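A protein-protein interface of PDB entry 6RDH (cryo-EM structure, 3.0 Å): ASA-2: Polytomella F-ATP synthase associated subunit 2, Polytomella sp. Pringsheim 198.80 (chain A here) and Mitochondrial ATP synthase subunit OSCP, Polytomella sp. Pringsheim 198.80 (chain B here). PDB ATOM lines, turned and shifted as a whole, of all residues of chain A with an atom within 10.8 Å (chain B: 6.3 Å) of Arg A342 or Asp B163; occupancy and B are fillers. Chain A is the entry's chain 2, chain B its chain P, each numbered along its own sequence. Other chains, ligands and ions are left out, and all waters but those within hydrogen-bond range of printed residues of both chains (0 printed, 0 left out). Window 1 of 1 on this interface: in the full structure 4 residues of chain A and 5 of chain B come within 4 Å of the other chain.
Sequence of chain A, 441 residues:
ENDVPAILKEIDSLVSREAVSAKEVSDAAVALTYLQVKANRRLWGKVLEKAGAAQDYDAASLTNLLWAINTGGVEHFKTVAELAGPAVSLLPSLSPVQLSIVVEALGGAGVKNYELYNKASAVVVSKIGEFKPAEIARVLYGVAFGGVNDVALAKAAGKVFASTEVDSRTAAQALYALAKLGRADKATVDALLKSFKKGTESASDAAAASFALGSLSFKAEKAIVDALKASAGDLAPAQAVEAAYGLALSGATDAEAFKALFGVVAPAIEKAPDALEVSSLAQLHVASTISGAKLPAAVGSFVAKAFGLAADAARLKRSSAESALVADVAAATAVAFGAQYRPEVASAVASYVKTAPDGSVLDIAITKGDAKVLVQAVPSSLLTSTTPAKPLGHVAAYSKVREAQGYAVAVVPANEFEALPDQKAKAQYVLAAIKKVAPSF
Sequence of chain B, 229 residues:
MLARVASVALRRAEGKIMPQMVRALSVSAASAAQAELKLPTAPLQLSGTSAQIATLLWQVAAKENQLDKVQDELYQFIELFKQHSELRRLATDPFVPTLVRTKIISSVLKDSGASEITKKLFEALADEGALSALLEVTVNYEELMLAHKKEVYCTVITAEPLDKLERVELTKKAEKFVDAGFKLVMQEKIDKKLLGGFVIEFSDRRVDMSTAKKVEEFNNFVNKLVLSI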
ATOM      1  N   ALA A 330      34.596   0.740   1.788  1.00  0.00           N
ATOM      2  CA  ALA A 330      33.871   1.552   2.757  1.00  0.00           C
ATOM      3  C   ALA A 330      33.429   0.726   3.959  1.00  0.00           C
ATOM      4  O   ALA A 330      33.444   1.217   5.093  1.00  0.00           O
ATOM      5  CB  ALA A 330      32.676   2.226   2.090  1.00  0.00           C
ATOM      6  N   ALA A 331      33.067  -0.540   3.742  1.00  0.00           N
ATOM      7  CA  ALA A 331      32.777  -1.427   4.868  1.00  0.00           C
ATOM      8  C   ALA A 331      34.031  -1.715   5.684  1.00  0.00           C
ATOM      9  O   ALA A 331      33.969  -1.832   6.915  1.00  0.00           O
ATOM     10  CB  ALA A 331      32.160  -2.729   4.369  1.00  0.00           C
ATOM     11  N   ALA A 334      34.568   1.182   7.804  1.00  0.00           N
ATOM     12  CA  ALA A 334      33.641   1.133   8.929  1.00  0.00           C
ATOM     13  C   ALA A 334      34.176   0.231  10.035  1.00  0.00           C
ATOM     14  O   ALA A 334      34.279   0.647  11.193  1.00  0.00           O
ATOM     15  CB  ALA A 334      32.266   0.663   8.462  1.00  0.00           C
ATOM     16  N   VAL A 335      34.574  -0.999   9.689  1.00  0.00           N
ATOM     17  CA  VAL A 335      35.116  -1.904  10.702  1.00  0.00           C
ATOM     18  C   VAL A 335      36.590  -1.670  10.985  1.00  0.00           C
ATOM     19  O   VAL A 335      37.203  -2.466  11.708  1.00  0.00           O
ATOM     20  CB  VAL A 335      34.884  -3.384  10.335  1.00  0.00           C
ATOM     21  CG1 VAL A 335      33.421  -3.643  10.168  1.00  0.00           C
ATOM     22  CG2 VAL A 335      35.593  -3.744   9.067  1.00  0.00           C
ATOM     23  N   GLY A 338      36.037   1.221  13.871  1.00  0.00           N
ATOM     24  CA  GLY A 338      35.275   0.704  14.983  1.00  0.00           C
ATOM     25  C   GLY A 338      33.792   0.687  14.689  1.00  0.00           C
ATOM     26  O   GLY A 338      33.101   1.697  14.848  1.00  0.00           O
ATOM     27  N   ALA A 339      33.301  -0.479  14.268  1.00  0.00           N
ATOM     28  CA  ALA A 339      31.880  -0.689  14.002  1.00  0.00           C
ATOM     29  C   ALA A 339      31.669  -2.197  14.084  1.00  0.00           C
ATOM     30  O   ALA A 339      31.995  -2.917  13.139  1.00  0.00           O
ATOM     31  CB  ALA A 339      31.469  -0.141  12.647  1.00  0.00           C
ATOM     32  N   GLN A 340      31.143  -2.660  15.213  1.00  0.00           N
ATOM     33  CA  GLN A 340      31.140  -4.093  15.466  1.00  0.00           C
ATOM     34  C   GLN A 340      30.052  -4.813  14.686  1.00  0.00           C
ATOM     35  O   GLN A 340      30.258  -5.951  14.253  1.00  0.00           O
ATOM     36  CB  GLN A 340      30.986  -4.354  16.965  1.00  0.00           C
ATOM     37  CG  GLN A 340      31.227  -5.796  17.384  1.00  0.00           C
ATOM     38  CD  GLN A 340      32.412  -6.425  16.682  1.00  0.00           C
ATOM     39  OE1 GLN A 340      32.255  -7.341  15.879  1.00  0.00           O
ATOM     40  NE2 GLN A 340      33.609  -5.946  16.994  1.00  0.00           N
ATOM     41  N   TYR A 341      28.912  -4.171  14.474  1.00  0.00           N
ATOM     42  CA  TYR A 341      27.759  -4.839  13.903  1.00  0.00           C
ATOM     43  C   TYR A 341      27.296  -4.127  12.641  1.00  0.00           C
ATOM     44  O   TYR A 341      27.645  -2.973  12.382  1.00  0.00           O
ATOM     45  CB  TYR A 341      26.626  -4.924  14.927  1.00  0.00           C
ATOM     46  CG  TYR A 341      27.082  -5.512  16.240  1.00  0.00           C
ATOM     47  CD1 TYR A 341      27.428  -6.855  16.333  1.00  0.00           C
ATOM     48  CD2 TYR A 341      27.185  -4.725  17.382  1.00  0.00           C
ATOM     49  CE1 TYR A 341      27.854  -7.405  17.523  1.00  0.00           C
ATOM     50  CE2 TYR A 341      27.613  -5.265  18.581  1.00  0.00           C
ATOM     51  CZ  TYR A 341      27.948  -6.607  18.642  1.00  0.00           C
ATOM     52  OH  TYR A 341      28.375  -7.160  19.825  1.00  0.00           O
ATOM     53  N   ARG A 342      26.493  -4.848  11.861  1.00  0.00           N
ATOM     54  CA  ARG A 342      26.071  -4.361  10.551  1.00  0.00           C
ATOM     55  C   ARG A 342      25.188  -3.109  10.531  1.00  0.00           C
ATOM     56  O   ARG A 342      25.276  -2.380   9.526  1.00  0.00           O
ATOM     57  CB  ARG A 342      25.384  -5.506   9.797  1.00  0.00           C
ATOM     58  CG  ARG A 342      26.296  -6.683   9.543  1.00  0.00           C
ATOM     59  CD  ARG A 342      25.621  -7.707   8.668  1.00  0.00           C
ATOM     60  NE  ARG A 342      24.530  -8.374   9.368  1.00  0.00           N
ATOM     61  CZ  ARG A 342      24.584  -9.631   9.787  1.00  0.00           C
ATOM     62  NH1 ARG A 342      23.553 -10.168  10.423  1.00  0.00           N
ATOM     63  NH2 ARG A 342      25.665 -10.358   9.555  1.00  0.00           N
ATOM     64  N   PRO A 343      24.320  -2.809  11.519  1.00  0.00           N
ATOM     65  CA  PRO A 343      23.662  -1.487  11.499  1.00  0.00           C
ATOM     66  C   PRO A 343      24.616  -0.308  11.563  1.00  0.00           C
ATOM     67  O   PRO A 343      24.471   0.640  10.781  1.00  0.00           O
ATOM     68  CB  PRO A 343      22.747  -1.548  12.722  1.00  0.00           C
ATOM     69  CG  PRO A 343      22.346  -2.929  12.772  1.00  0.00           C
ATOM     70  CD  PRO A 343      23.565  -3.718  12.405  1.00  0.00           C
ATOM     71  N   GLU A 344      25.608  -0.340  12.448  1.00  0.00           N
ATOM     72  CA  GLU A 344      26.545   0.771  12.469  1.00  0.00           C
ATOM     73  C   GLU A 344      27.578   0.685  11.353  1.00  0.00           C
ATOM     74  O   GLU A 344      28.139   1.722  10.990  1.00  0.00           O
ATOM     75  CB  GLU A 344      27.222   0.890  13.837  1.00  0.00           C
ATOM     76  CG  GLU A 344      28.117  -0.253  14.222  1.00  0.00           C
ATOM     77  CD  GLU A 344      27.447  -1.215  15.163  1.00  0.00           C
ATOM     78  OE1 GLU A 344      26.247  -1.479  14.970  1.00  0.00           O
ATOM     79  OE2 GLU A 344      28.116  -1.700  16.097  1.00  0.00           O
ATOM     80  N   VAL A 345      27.798  -0.500  10.769  1.00  0.00           N
ATOM     81  CA  VAL A 345      28.568  -0.594   9.525  1.00  0.00           C
ATOM     82  C   VAL A 345      27.871   0.184   8.419  1.00  0.00           C
ATOM     83  O   VAL A 345      28.477   1.038   7.760  1.00  0.00           O
ATOM     84  CB  VAL A 345      28.778  -2.066   9.122  1.00  0.00           C
ATOM     85  CG1 VAL A 345      29.140  -2.187   7.654  1.00  0.00           C
ATOM     86  CG2 VAL A 345      29.856  -2.695   9.947  1.00  0.00           C
ATOM     87  N   ALA A 346      26.574  -0.077   8.226  1.00  0.00           N
ATOM     88  CA  ALA A 346      25.820   0.602   7.179  1.00  0.00           C
ATOM     89  C   ALA A 346      25.657   2.087   7.478  1.00  0.00           C
ATOM     90  O   ALA A 346      25.689   2.915   6.559  1.00  0.00           O
ATOM     91  CB  ALA A 346      24.458  -0.065   7.005  1.00  0.00           C
ATOM     92  N   SER A 347      25.524   2.445   8.757  1.00  0.00           N
ATOM     93  CA  SER A 347      25.384   3.850   9.117  1.00  0.00           C
ATOM     94  C   SER A 347      26.686   4.609   8.906  1.00  0.00           C
ATOM     95  O   SER A 347      26.671   5.750   8.431  1.00  0.00           O
ATOM     96  CB  SER A 347      24.920   3.975  10.566  1.00  0.00           C
ATOM     97  OG  SER A 347      24.967   5.322  10.998  1.00  0.00           O
ATOM     98  N   ALA A 348      27.823   3.973   9.198  1.00  0.00           N
ATOM     99  CA  ALA A 348      29.110   4.604   8.938  1.00  0.00           C
ATOM    100  C   ALA A 348      29.366   4.753   7.444  1.00  0.00           C
ATOM    101  O   ALA A 348      29.814   5.817   6.999  1.00  0.00           O
ATOM    102  CB  ALA A 348      30.225   3.797   9.595  1.00  0.00           C
ATOM    103  N   VAL A 349      29.069   3.708   6.659  1.00  0.00           N
ATOM    104  CA  VAL A 349      29.282   3.756   5.212  1.00  0.00           C
ATOM    105  C   VAL A 349      28.413   4.831   4.577  1.00  0.00           C
ATOM    106  O   VAL A 349      28.886   5.620   3.755  1.00  0.00           O
ATOM    107  CB  VAL A 349      29.029   2.372   4.585  1.00  0.00           C
ATOM    108  CG1 VAL A 349      28.959   2.464   3.082  1.00  0.00           C
ATOM    109  CG2 VAL A 349      30.120   1.422   4.967  1.00  0.00           C
ATOM    110  N   ALA A 350      27.152   4.932   5.000  1.00  0.00           N
ATOM    111  CA  ALA A 350      26.303   6.007   4.507  1.00  0.00           C
ATOM    112  C   ALA A 350      26.714   7.371   5.045  1.00  0.00           C
ATOM    113  O   ALA A 350      26.358   8.389   4.446  1.00  0.00           O
ATOM    114  CB  ALA A 350      24.846   5.731   4.865  1.00  0.00           C
ATOM    115  N   SER A 351      27.443   7.417   6.160  1.00  0.00           N
ATOM    116  CA  SER A 351      27.950   8.689   6.655  1.00  0.00           C
ATOM    117  C   SER A 351      29.167   9.162   5.876  1.00  0.00           C
ATOM    118  O   SER A 351      29.405  10.371   5.784  1.00  0.00           O
ATOM    119  CB  SER A 351      28.299   8.568   8.136  1.00  0.00           C
ATOM    120  OG  SER A 351      27.206   8.047   8.867  1.00  0.00           O
ATOM    121  N   ASP A 422      39.717 -11.848   4.674  1.00  0.00           N
ATOM    122  CA  ASP A 422      38.382 -11.466   5.098  1.00  0.00           C
ATOM    123  C   ASP A 422      38.414 -10.027   5.600  1.00  0.00           C
ATOM    124  O   ASP A 422      39.394  -9.303   5.405  1.00  0.00           O
ATOM    125  CB  ASP A 422      37.856 -12.443   6.156  1.00  0.00           C
ATOM    126  CG  ASP A 422      36.351 -12.612   6.091  1.00  0.00           C
ATOM    127  OD1 ASP A 422      35.895 -13.701   5.678  1.00  0.00           O
ATOM    128  OD2 ASP A 422      35.628 -11.651   6.432  1.00  0.00           O
ATOM    129  N   GLN A 423      37.331  -9.624   6.266  1.00  0.00           N
ATOM    130  CA  GLN A 423      37.075  -8.214   6.523  1.00  0.00           C
ATOM    131  C   GLN A 423      37.986  -7.649   7.602  1.00  0.00           C
ATOM    132  O   GLN A 423      38.218  -6.437   7.635  1.00  0.00           O
ATOM    133  CB  GLN A 423      35.610  -8.030   6.912  1.00  0.00           C
ATOM    134  CG  GLN A 423      35.062  -6.632   6.716  1.00  0.00           C
ATOM    135  CD  GLN A 423      33.625  -6.514   7.168  1.00  0.00           C
ATOM    136  OE1 GLN A 423      33.100  -5.416   7.323  1.00  0.00           O
ATOM    137  NE2 GLN A 423      32.979  -7.650   7.378  1.00  0.00           N
ATOM    138  N   GLU B 160      20.022 -13.579   7.059  1.00  0.00           N
ATOM    139  CA  GLU B 160      21.235 -14.142   7.628  1.00  0.00           C
ATOM    140  C   GLU B 160      21.089 -14.075   9.140  1.00  0.00           C
ATOM    141  O   GLU B 160      20.272 -13.298   9.646  1.00  0.00           O
ATOM    142  CB  GLU B 160      22.484 -13.382   7.151  1.00  0.00           C
ATOM    143  CG  GLU B 160      22.659 -11.989   7.728  1.00  0.00           C
ATOM    144  CD  GLU B 160      22.036 -10.906   6.874  1.00  0.00           C
ATOM    145  OE1 GLU B 160      21.232 -11.235   5.984  1.00  0.00           O
ATOM    146  OE2 GLU B 160      22.355  -9.719   7.088  1.00  0.00           O
ATOM    147  N   PRO B 161      21.817 -14.922   9.886  1.00  0.00           N
ATOM    148  CA  PRO B 161      21.716 -14.889  11.352  1.00  0.00           C
ATOM    149  C   PRO B 161      22.140 -13.551  11.936  1.00  0.00           C
ATOM    150  O   PRO B 161      23.036 -12.875  11.427  1.00  0.00           O
ATOM    151  CB  PRO B 161      22.658 -16.010  11.796  1.00  0.00           C
ATOM    152  CG  PRO B 161      22.623 -16.969  10.679  1.00  0.00           C
ATOM    153  CD  PRO B 161      22.511 -16.143   9.431  1.00  0.00           C
ATOM    154  N   LEU B 162      21.467 -13.175  13.016  1.00  0.00           N
ATOM    155  CA  LEU B 162      21.433 -11.790  13.454  1.00  0.00           C
ATOM    156  C   LEU B 162      22.661 -11.411  14.269  1.00  0.00           C
ATOM    157  O   LEU B 162      23.343 -12.258  14.852  1.00  0.00           O
ATOM    158  CB  LEU B 162      20.178 -11.530  14.284  1.00  0.00           C
ATOM    159  CG  LEU B 162      18.848 -11.475  13.540  1.00  0.00           C
ATOM    160  CD1 LEU B 162      18.153 -12.821  13.555  1.00  0.00           C
ATOM    161  CD2 LEU B 162      17.966 -10.420  14.155  1.00  0.00           C
ATOM    162  N   ASP B 163      22.940 -10.114  14.289  1.00  0.00           N
ATOM    163  CA  ASP B 163      23.832  -9.515  15.263  1.00  0.00           C
ATOM    164  C   ASP B 163      23.026  -9.095  16.484  1.00  0.00           C
ATOM    165  O   ASP B 163      21.796  -9.096  16.473  1.00  0.00           O
ATOM    166  CB  ASP B 163      24.559  -8.313  14.662  1.00  0.00           C
ATOM    167  CG  ASP B 163      25.387  -8.682  13.455  1.00  0.00           C
ATOM    168  OD1 ASP B 163      25.586  -9.892  13.221  1.00  0.00           O
ATOM    169  OD2 ASP B 163      25.840  -7.765  12.741  1.00  0.00           O
ATOM    170  N   LYS B 164      23.729  -8.722  17.549  1.00  0.00           N
ATOM    171  CA  LYS B 164      23.011  -8.363  18.760  1.00  0.00           C
ATOM    172  C   LYS B 164      22.526  -6.920  18.747  1.00  0.00           C
ATOM    173  O   LYS B 164      21.872  -6.500  19.706  1.00  0.00           O
ATOM    174  CB  LYS B 164      23.872  -8.654  19.998  1.00  0.00           C
ATOM    175  CG  LYS B 164      24.182 -10.110  20.317  1.00  0.00           C
ATOM    176  CD  LYS B 164      25.065 -10.238  21.558  1.00  0.00           C
ATOM    177  CE  LYS B 164      25.357 -11.685  21.892  1.00  0.00           C
ATOM    178  NZ  LYS B 164      26.235 -11.801  23.086  1.00  0.00           N
ATOM    179  N   LEU B 165      22.835  -6.150  17.703  1.00  0.00           N
ATOM    180  CA  LEU B 165      22.151  -4.879  17.500  1.00  0.00           C
ATOM    181  C   LEU B 165      21.048  -4.984  16.455  1.00  0.00           C
ATOM    182  O   LEU B 165      20.043  -4.265  16.553  1.00  0.00           O
ATOM    183  CB  LEU B 165      23.144  -3.784  17.105  1.00  0.00           C
ATOM    184  CG  LEU B 165      22.586  -2.367  17.296  1.00  0.00           C
ATOM    185  CD1 LEU B 165      22.178  -2.147  18.747  1.00  0.00           C
ATOM    186  CD2 LEU B 165      23.558  -1.298  16.858  1.00  0.00           C
ATOM    187  N   GLU B 166      21.211  -5.871  15.464  1.00  0.00           N
ATOM    188  CA  GLU B 166      20.098  -6.226  14.585  1.00  0.00           C
ATOM    189  C   GLU B 166      18.938  -6.793  15.379  1.00  0.00           C
ATOM    190  O   GLU B 166      17.782  -6.448  15.123  1.00  0.00           O
ATOM    191  CB  GLU B 166      20.531  -7.235  13.524  1.00  0.00           C
ATOM    192  CG  GLU B 166      21.351  -6.666  12.389  1.00  0.00           C
ATOM    193  CD  GLU B 166      21.711  -7.718  11.355  1.00  0.00           C
ATOM    194  OE1 GLU B 166      21.444  -8.911  11.601  1.00  0.00           O
ATOM    195  OE2 GLU B 166      22.257  -7.358  10.293  1.00  0.00           O
ATOM    196  N   ARG B 167      19.236  -7.631  16.376  1.00  0.00           N
ATOM    197  CA  ARG B 167      18.196  -8.194  17.229  1.00  0.00           C
ATOM    198  C   ARG B 167      17.503  -7.118  18.049  1.00  0.00           C
ATOM    199  O   ARG B 167      16.272  -7.102  18.146  1.00  0.00           O
ATOM    200  CB  ARG B 167      18.806  -9.250  18.143  1.00  0.00           C
ATOM    201  CG  ARG B 167      17.816  -9.943  19.041  1.00  0.00           C
ATOM    202  CD  ARG B 167      18.450 -11.145  19.716  1.00  0.00           C
ATOM    203  NE  ARG B 167      18.593 -12.286  18.814  1.00  0.00           N
ATOM    204  CZ  ARG B 167      19.734 -12.644  18.233  1.00  0.00           C
ATOM    205  NH1 ARG B 167      20.835 -11.946  18.452  1.00  0.00           N
ATOM    206  NH2 ARG B 167      19.771 -13.697  17.430  1.00  0.00           N
ATOM    207  N   VAL B 168      18.271  -6.173  18.592  1.00  0.00           N
ATOM    208  CA  VAL B 168      17.697  -5.166  19.478  1.00  0.00           C
ATOM    209  C   VAL B 168      16.860  -4.162  18.691  1.00  0.00           C
ATOM    210  O   VAL B 168      15.723  -3.850  19.067  1.00  0.00           O
ATOM    211  CB  VAL B 168      18.816  -4.492  20.292  1.00  0.00           C
ATOM    212  CG1 VAL B 168      18.376  -3.142  20.838  1.00  0.00           C
ATOM    213  CG2 VAL B 168      19.247  -5.409  21.428  1.00  0.00           C
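Among the printed residues, merely in contact across the chains: Glu A344 with Leu B165 (3.3 Å), Tyr A341 with Asp B163 (3.6 Å) and Pro A343 with Glu B166 (3.7 Å).
Among the printed residues, 7 pairs touch across the chains.
Among the printed residues, Asp or Glu carboxylates within 4 Å of a Lys or Arg side-chain nitrogen of the other chain: Arg A342 with Glu B160, Arg A342 with Asp B163 and Arg A342 with Glu B166.
N of Asp B163 is in hydrogen-bond range of OE1 of Glu B166 (3.3 Å).
The backbone NH of Gln A340 sits at hydrogen-bond distance from the side-chain carboxylate of Glu A344 (3.3 Å).
N of Tyr A341 is in hydrogen-bond range of OE2 of Glu A344 (3.1 Å).
The guanidinium group (NE) of Arg A342 is in salt-bridge range of the side-chain carboxylate (OE2) of Glu B166, 2.7 Å away.
The backbone carbonyl oxygen of Pro B161 sits at hydrogen-bond distance from the guanidinium group of Arg A342, at 2.9 Å.
OD1 of Asp B163 lies within salt-bridge range of NH1 of Arg A342 (3.5 Å).
The side-chain carboxylate of Glu B160 lies within salt-bridge range of the guanidinium group of Arg A342, 3.4 Å away.
Gly A338 touches none of the printed residues of chain B.
Of the printed residues of chain B, Tyr A341 touches Asp B163.
Arg A342 touches just these residues of chain B: Glu B160, Pro B161, Asp B163 and Glu B166.
Printed residues of chain B within 4 Å of Glu A344: Leu B165.
Ser A351 touches none of the printed residues of chain B.
Printed residues of chain A within 4 Å of Glu B160: Arg A342 (3.4 Å).
Of the printed residues of chain A, Pro B161 touches Arg A342 (2.9 Å).
No residue of chain A comes within 4 Å of Leu B162.
Of the printed residues of chain A, Asp B163 touches Tyr A341 (3.6 Å) and Arg A342 (3.1 Å).
Printed residues of chain A within 4 Å of Leu B165: Glu A344.
Of chain A, only Arg A342 (2.7 Å) and Pro A343 (3.7 Å) come within 4 Å of Glu B166.
The nearest residue of chain A that does not touch Asp B163 is Pro A343 (4.7 Å).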
